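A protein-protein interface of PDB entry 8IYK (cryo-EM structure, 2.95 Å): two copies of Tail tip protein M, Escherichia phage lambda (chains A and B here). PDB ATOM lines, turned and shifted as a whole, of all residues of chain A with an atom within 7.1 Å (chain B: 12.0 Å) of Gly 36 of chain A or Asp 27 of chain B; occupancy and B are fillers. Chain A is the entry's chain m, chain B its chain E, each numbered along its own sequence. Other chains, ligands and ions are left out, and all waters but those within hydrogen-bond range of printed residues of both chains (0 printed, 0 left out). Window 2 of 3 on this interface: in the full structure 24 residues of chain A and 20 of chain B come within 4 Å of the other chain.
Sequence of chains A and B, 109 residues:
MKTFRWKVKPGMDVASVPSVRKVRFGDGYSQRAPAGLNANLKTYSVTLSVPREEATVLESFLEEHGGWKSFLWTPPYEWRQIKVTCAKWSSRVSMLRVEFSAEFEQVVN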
ATOM      1  N   SER A  19       1.597  19.017 -19.599  1.00  0.00           N
ATOM      2  CA  SER A  19       2.321  20.248 -19.889  1.00  0.00           C
ATOM      3  C   SER A  19       2.773  20.239 -21.343  1.00  0.00           C
ATOM      4  O   SER A  19       3.562  19.378 -21.748  1.00  0.00           O
ATOM      5  CB  SER A  19       3.522  20.398 -18.954  1.00  0.00           C
ATOM      6  OG  SER A  19       4.103  19.138 -18.673  1.00  0.00           O
ATOM      7  N   VAL A  20       2.271  21.196 -22.125  1.00  0.00           N
ATOM      8  CA  VAL A  20       2.613  21.331 -23.533  1.00  0.00           C
ATOM      9  C   VAL A  20       2.991  22.781 -23.809  1.00  0.00           C
ATOM     10  O   VAL A  20       2.677  23.689 -23.038  1.00  0.00           O
ATOM     11  CB  VAL A  20       1.465  20.892 -24.468  1.00  0.00           C
ATOM     12  CG1 VAL A  20       0.738  19.689 -23.900  1.00  0.00           C
ATOM     13  CG2 VAL A  20       0.494  22.038 -24.698  1.00  0.00           C
ATOM     14  N   ARG A  21       3.685  22.985 -24.926  1.00  0.00           N
ATOM     15  CA  ARG A  21       4.019  24.316 -25.413  1.00  0.00           C
ATOM     16  C   ARG A  21       2.996  24.714 -26.468  1.00  0.00           C
ATOM     17  O   ARG A  21       2.866  24.041 -27.494  1.00  0.00           O
ATOM     18  CB  ARG A  21       5.432  24.355 -25.993  1.00  0.00           C
ATOM     19  CG  ARG A  21       6.530  24.098 -24.982  1.00  0.00           C
ATOM     20  CD  ARG A  21       7.866  24.629 -25.472  1.00  0.00           C
ATOM     21  NE  ARG A  21       8.904  23.607 -25.461  1.00  0.00           N
ATOM     22  CZ  ARG A  21       9.303  22.933 -26.532  1.00  0.00           C
ATOM     23  NH1 ARG A  21       8.768  23.147 -27.722  1.00  0.00           N
ATOM     24  NH2 ARG A  21      10.263  22.023 -26.403  1.00  0.00           N
ATOM     25  N   ALA A  33       3.413  21.697 -29.074  1.00  0.00           N
ATOM     26  CA  ALA A  33       4.596  20.873 -28.908  1.00  0.00           C
ATOM     27  C   ALA A  33       4.527  20.132 -27.582  1.00  0.00           C
ATOM     28  O   ALA A  33       3.933  20.629 -26.619  1.00  0.00           O
ATOM     29  CB  ALA A  33       5.875  21.722 -28.960  1.00  0.00           C
ATOM     30  N   PRO A  34       5.135  18.945 -27.499  1.00  0.00           N
ATOM     31  CA  PRO A  34       5.029  18.139 -26.272  1.00  0.00           C
ATOM     32  C   PRO A  34       5.774  18.707 -25.075  1.00  0.00           C
ATOM     33  O   PRO A  34       5.674  18.126 -23.987  1.00  0.00           O
ATOM     34  CB  PRO A  34       5.626  16.788 -26.693  1.00  0.00           C
ATOM     35  CG  PRO A  34       6.491  17.102 -27.862  1.00  0.00           C
ATOM     36  CD  PRO A  34       5.802  18.208 -28.584  1.00  0.00           C
ATOM     37  N   ALA A  35       6.515  19.804 -25.233  1.00  0.00           N
ATOM     38  CA  ALA A  35       7.233  20.466 -24.137  1.00  0.00           C
ATOM     39  C   ALA A  35       8.241  19.482 -23.555  1.00  0.00           C
ATOM     40  O   ALA A  35       9.131  19.031 -24.296  1.00  0.00           O
ATOM     41  CB  ALA A  35       6.222  21.040 -23.142  1.00  0.00           C
ATOM     42  N   GLY A  36       8.155  19.124 -22.277  1.00  0.00           N
ATOM     43  CA  GLY A  36       9.152  18.284 -21.654  1.00  0.00           C
ATOM     44  C   GLY A  36       9.026  16.824 -22.038  1.00  0.00           C
ATOM     45  O   GLY A  36       8.256  16.433 -22.914  1.00  0.00           O
ATOM     46  N   LEU A  37       9.815  16.000 -21.349  1.00  0.00           N
ATOM     47  CA  LEU A  37       9.859  14.567 -21.608  1.00  0.00           C
ATOM     48  C   LEU A  37       8.888  13.794 -20.726  1.00  0.00           C
ATOM     49  O   LEU A  37       8.249  12.845 -21.192  1.00  0.00           O
ATOM     50  CB  LEU A  37      11.284  14.047 -21.408  1.00  0.00           C
ATOM     51  CG  LEU A  37      11.577  12.560 -21.570  1.00  0.00           C
ATOM     52  CD1 LEU A  37      11.967  12.258 -23.004  1.00  0.00           C
ATOM     53  CD2 LEU A  37      12.681  12.147 -20.615  1.00  0.00           C
ATOM     54  N   ASN A  38       8.765  14.180 -19.456  1.00  0.00           N
ATOM     55  CA  ASN A  38       7.788  13.579 -18.550  1.00  0.00           C
ATOM     56  C   ASN A  38       6.559  14.483 -18.539  1.00  0.00           C
ATOM     57  O   ASN A  38       6.351  15.302 -17.641  1.00  0.00           O
ATOM     58  CB  ASN A  38       8.384  13.397 -17.161  1.00  0.00           C
ATOM     59  CG  ASN A  38       9.082  12.064 -17.000  1.00  0.00           C
ATOM     60  OD1 ASN A  38      10.186  11.991 -16.462  1.00  0.00           O
ATOM     61  ND2 ASN A  38       8.441  11.001 -17.466  1.00  0.00           N
ATOM     62  N   ALA A  39       5.734  14.321 -19.574  1.00  0.00           N
ATOM     63  CA  ALA A  39       4.655  15.252 -19.887  1.00  0.00           C
ATOM     64  C   ALA A  39       3.676  15.447 -18.736  1.00  0.00           C
ATOM     65  O   ALA A  39       3.573  16.548 -18.188  1.00  0.00           O
ATOM     66  CB  ALA A  39       3.901  14.780 -21.132  1.00  0.00           C
ATOM     67  N   VAL A 108       9.316  12.059 -10.293  1.00  0.00           N
ATOM     68  CA  VAL A 108      10.254  11.254 -11.065  1.00  0.00           C
ATOM     69  C   VAL A 108      11.520  10.958 -10.270  1.00  0.00           C
ATOM     70  O   VAL A 108      11.931   9.801 -10.144  1.00  0.00           O
ATOM     71  CB  VAL A 108      10.601  11.932 -12.409  1.00  0.00           C
ATOM     72  CG1 VAL A 108      11.819  11.279 -13.035  1.00  0.00           C
ATOM     73  CG2 VAL A 108       9.413  11.868 -13.348  1.00  0.00           C
ATOM     74  N   VAL B  23      11.966  23.166  -6.231  1.00  0.00           N
ATOM     75  CA  VAL B  23      12.453  23.669  -7.507  1.00  0.00           C
ATOM     76  C   VAL B  23      12.036  22.671  -8.572  1.00  0.00           C
ATOM     77  O   VAL B  23      12.262  21.466  -8.419  1.00  0.00           O
ATOM     78  CB  VAL B  23      13.982  23.852  -7.503  1.00  0.00           C
ATOM     79  CG1 VAL B  23      14.453  24.417  -8.831  1.00  0.00           C
ATOM     80  CG2 VAL B  23      14.403  24.746  -6.352  1.00  0.00           C
ATOM     81  N   ARG B  24      11.420  23.162  -9.637  1.00  0.00           N
ATOM     82  CA  ARG B  24      10.962  22.312 -10.725  1.00  0.00           C
ATOM     83  C   ARG B  24      11.898  22.495 -11.909  1.00  0.00           C
ATOM     84  O   ARG B  24      11.926  23.561 -12.532  1.00  0.00           O
ATOM     85  CB  ARG B  24       9.515  22.620 -11.094  1.00  0.00           C
ATOM     86  CG  ARG B  24       8.997  21.817 -12.269  1.00  0.00           C
ATOM     87  CD  ARG B  24       7.464  21.808 -12.519  1.00  0.00           C
ATOM     88  NE  ARG B  24       6.584  21.320 -11.453  1.00  0.00           N
ATOM     89  CZ  ARG B  24       6.411  21.841 -10.243  1.00  0.00           C
ATOM     90  NH1 ARG B  24       6.883  23.033  -9.920  1.00  0.00           N
ATOM     91  NH2 ARG B  24       5.685  21.175  -9.351  1.00  0.00           N
ATOM     92  N   PHE B  25      12.657  21.446 -12.212  1.00  0.00           N
ATOM     93  CA  PHE B  25      13.566  21.409 -13.349  1.00  0.00           C
ATOM     94  C   PHE B  25      12.770  21.145 -14.617  1.00  0.00           C
ATOM     95  O   PHE B  25      11.551  21.339 -14.641  1.00  0.00           O
ATOM     96  CB  PHE B  25      14.649  20.348 -13.150  1.00  0.00           C
ATOM     97  CG  PHE B  25      15.634  20.689 -12.072  1.00  0.00           C
ATOM     98  CD1 PHE B  25      15.956  22.004 -11.803  1.00  0.00           C
ATOM     99  CD2 PHE B  25      16.230  19.694 -11.323  1.00  0.00           C
ATOM    100  CE1 PHE B  25      16.858  22.322 -10.809  1.00  0.00           C
ATOM    101  CE2 PHE B  25      17.134  20.005 -10.328  1.00  0.00           C
ATOM    102  CZ  PHE B  25      17.447  21.321 -10.072  1.00  0.00           C
ATOM    103  N   GLY B  26      13.436  20.692 -15.669  1.00  0.00           N
ATOM    104  CA  GLY B  26      12.816  20.663 -16.973  1.00  0.00           C
ATOM    105  C   GLY B  26      12.039  19.385 -17.193  1.00  0.00           C
ATOM    106  O   GLY B  26      10.915  19.257 -16.699  1.00  0.00           O
ATOM    107  N   ASP B  27      12.607  18.432 -17.922  1.00  0.00           N
ATOM    108  CA  ASP B  27      11.842  17.266 -18.343  1.00  0.00           C
ATOM    109  C   ASP B  27      11.490  16.342 -17.182  1.00  0.00           C
ATOM    110  O   ASP B  27      11.979  15.211 -17.107  1.00  0.00           O
ATOM    111  CB  ASP B  27      12.622  16.496 -19.405  1.00  0.00           C
ATOM    112  CG  ASP B  27      13.127  17.389 -20.514  1.00  0.00           C
ATOM    113  OD1 ASP B  27      12.771  18.585 -20.519  1.00  0.00           O
ATOM    114  OD2 ASP B  27      13.873  16.899 -21.385  1.00  0.00           O
ATOM    115  N   GLY B  28      10.630  16.814 -16.279  1.00  0.00           N
ATOM    116  CA  GLY B  28      10.052  15.985 -15.243  1.00  0.00           C
ATOM    117  C   GLY B  28      10.826  15.890 -13.947  1.00  0.00           C
ATOM    118  O   GLY B  28      10.344  15.247 -13.007  1.00  0.00           O
ATOM    119  N   TYR B  29      11.998  16.503 -13.856  1.00  0.00           N
ATOM    120  CA  TYR B  29      12.836  16.402 -12.672  1.00  0.00           C
ATOM    121  C   TYR B  29      12.614  17.597 -11.752  1.00  0.00           C
ATOM    122  O   TYR B  29      12.106  18.641 -12.163  1.00  0.00           O
ATOM    123  CB  TYR B  29      14.306  16.291 -13.074  1.00  0.00           C
ATOM    124  CG  TYR B  29      14.539  15.249 -14.144  1.00  0.00           C
ATOM    125  CD1 TYR B  29      14.545  13.898 -13.832  1.00  0.00           C
ATOM    126  CD2 TYR B  29      14.738  15.617 -15.466  1.00  0.00           C
ATOM    127  CE1 TYR B  29      14.751  12.942 -14.804  1.00  0.00           C
ATOM    128  CE2 TYR B  29      14.948  14.668 -16.446  1.00  0.00           C
ATOM    129  CZ  TYR B  29      14.951  13.332 -16.109  1.00  0.00           C
ATOM    130  OH  TYR B  29      15.158  12.383 -17.081  1.00  0.00           O
ATOM    131  N   SER B  30      12.994  17.427 -10.488  1.00  0.00           N
ATOM    132  CA  SER B  30      12.723  18.433  -9.470  1.00  0.00           C
ATOM    133  C   SER B  30      13.757  18.311  -8.357  1.00  0.00           C
ATOM    134  O   SER B  30      14.683  17.498  -8.423  1.00  0.00           O
ATOM    135  CB  SER B  30      11.301  18.293  -8.922  1.00  0.00           C
ATOM    136  OG  SER B  30      11.048  16.965  -8.500  1.00  0.00           O
ATOM    137  N   GLN B  31      13.587  19.137  -7.327  1.00  0.00           N
ATOM    138  CA  GLN B  31      14.517  19.188  -6.201  1.00  0.00           C
ATOM    139  C   GLN B  31      13.779  19.753  -4.996  1.00  0.00           C
ATOM    140  O   GLN B  31      13.263  20.873  -5.061  1.00  0.00           O
ATOM    141  CB  GLN B  31      15.733  20.040  -6.555  1.00  0.00           C
ATOM    142  CG  GLN B  31      16.441  20.668  -5.375  1.00  0.00           C
ATOM    143  CD  GLN B  31      17.425  21.738  -5.803  1.00  0.00           C
ATOM    144  OE1 GLN B  31      17.266  22.912  -5.469  1.00  0.00           O
ATOM    145  NE2 GLN B  31      18.444  21.339  -6.554  1.00  0.00           N
ATOM    146  N   ARG B  32      13.729  18.994  -3.902  1.00  0.00           N
ATOM    147  CA  ARG B  32      12.898  19.342  -2.756  1.00  0.00           C
ATOM    148  C   ARG B  32      13.718  19.358  -1.474  1.00  0.00           C
ATOM    149  O   ARG B  32      14.621  18.537  -1.293  1.00  0.00           O
ATOM    150  CB  ARG B  32      11.729  18.363  -2.612  1.00  0.00           C
ATOM    151  CG  ARG B  32      10.671  18.503  -3.691  1.00  0.00           C
ATOM    152  CD  ARG B  32       9.800  17.264  -3.787  1.00  0.00           C
ATOM    153  NE  ARG B  32      10.233  16.375  -4.856  1.00  0.00           N
ATOM    154  CZ  ARG B  32      10.894  15.242  -4.669  1.00  0.00           C
ATOM    155  NH1 ARG B  32      11.210  14.820  -3.456  1.00  0.00           N
ATOM    156  NH2 ARG B  32      11.247  14.514  -5.723  1.00  0.00           N
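Among the printed residues, pairs that only touch across the chains: Gly 36 of chain A with Asp 27 of chain B, Leu 37 of chain A with Asp 27 of chain B, Asn 38 of chain A with Asp 27 of chain B, Asn 38 of chain A with Gly 28 of chain B, Val 108 of chain A with Gly 28 of chain B and Val 108 of chain A with Tyr 29 of chain B.
No residue of chain B comes within 4 Å of Ser 19 of chain A.
No residue of chain B comes within 4 Å of Pro 34 of chain A.
No residue of chain B comes within 4 Å of Ala 35 of chain A.
Gly 36 of chain A touches one residue of chain B.
Of chain B, only Asp 27 (3.4 Å) comes within 4 Å of Leu 37 of chain A.
Of the printed residues of chain B, Asn 38 of chain A touches Asp 27 and Gly 28.
Ala 39 of chain A touches none of the printed residues of chain B.
Printed residues of chain B within 4 Å of Val 108 of chain A: Gly 28 and Tyr 29.
Of the printed residues of chain A, Asp 27 of chain B touches Gly 36 (3.8 Å), Leu 37 (3.4 Å) and Asn 38 (3.7 Å).
Of the printed residues of chain A, Gly 28 of chain B touches Asn 38 (3.6 Å) and Val 108 (3.4 Å).
The nearest residue of chain B that does not touch Gly 36 of chain A is Gly 26 of chain B (5.3 Å).
The nearest residue of chain A that does not touch Asp 27 of chain B is Ala 35 of chain A (5.3 Å).
The nearest printed residue of chain A that does not touch Tyr 29 of chain B is Leu 37 of chain A (4.3 Å).
Hydrophobic or aromatic side chains of chain A within 4 Å of the printed part of chain B: Leu 37 and Val 108.
Of the 10 printed residues of chain B, 3 touch a printed residue of chain A.
Hydrophobic or aromatic side chains of chain B within 4 Å of the printed part of chain A: Tyr 29.
Along chain B the printed residues that touch a printed residue of chain A span positions 27 to 29.
Among the printed residues, no Asp or Glu carboxylate lies within 4 Å of a Lys or Arg side-chain nitrogen of the other chain.
No position is printed for both chains.
Of the 6 pairs that touch across the chains among the printed residues, none has its exchanged pair printed and touching as well.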
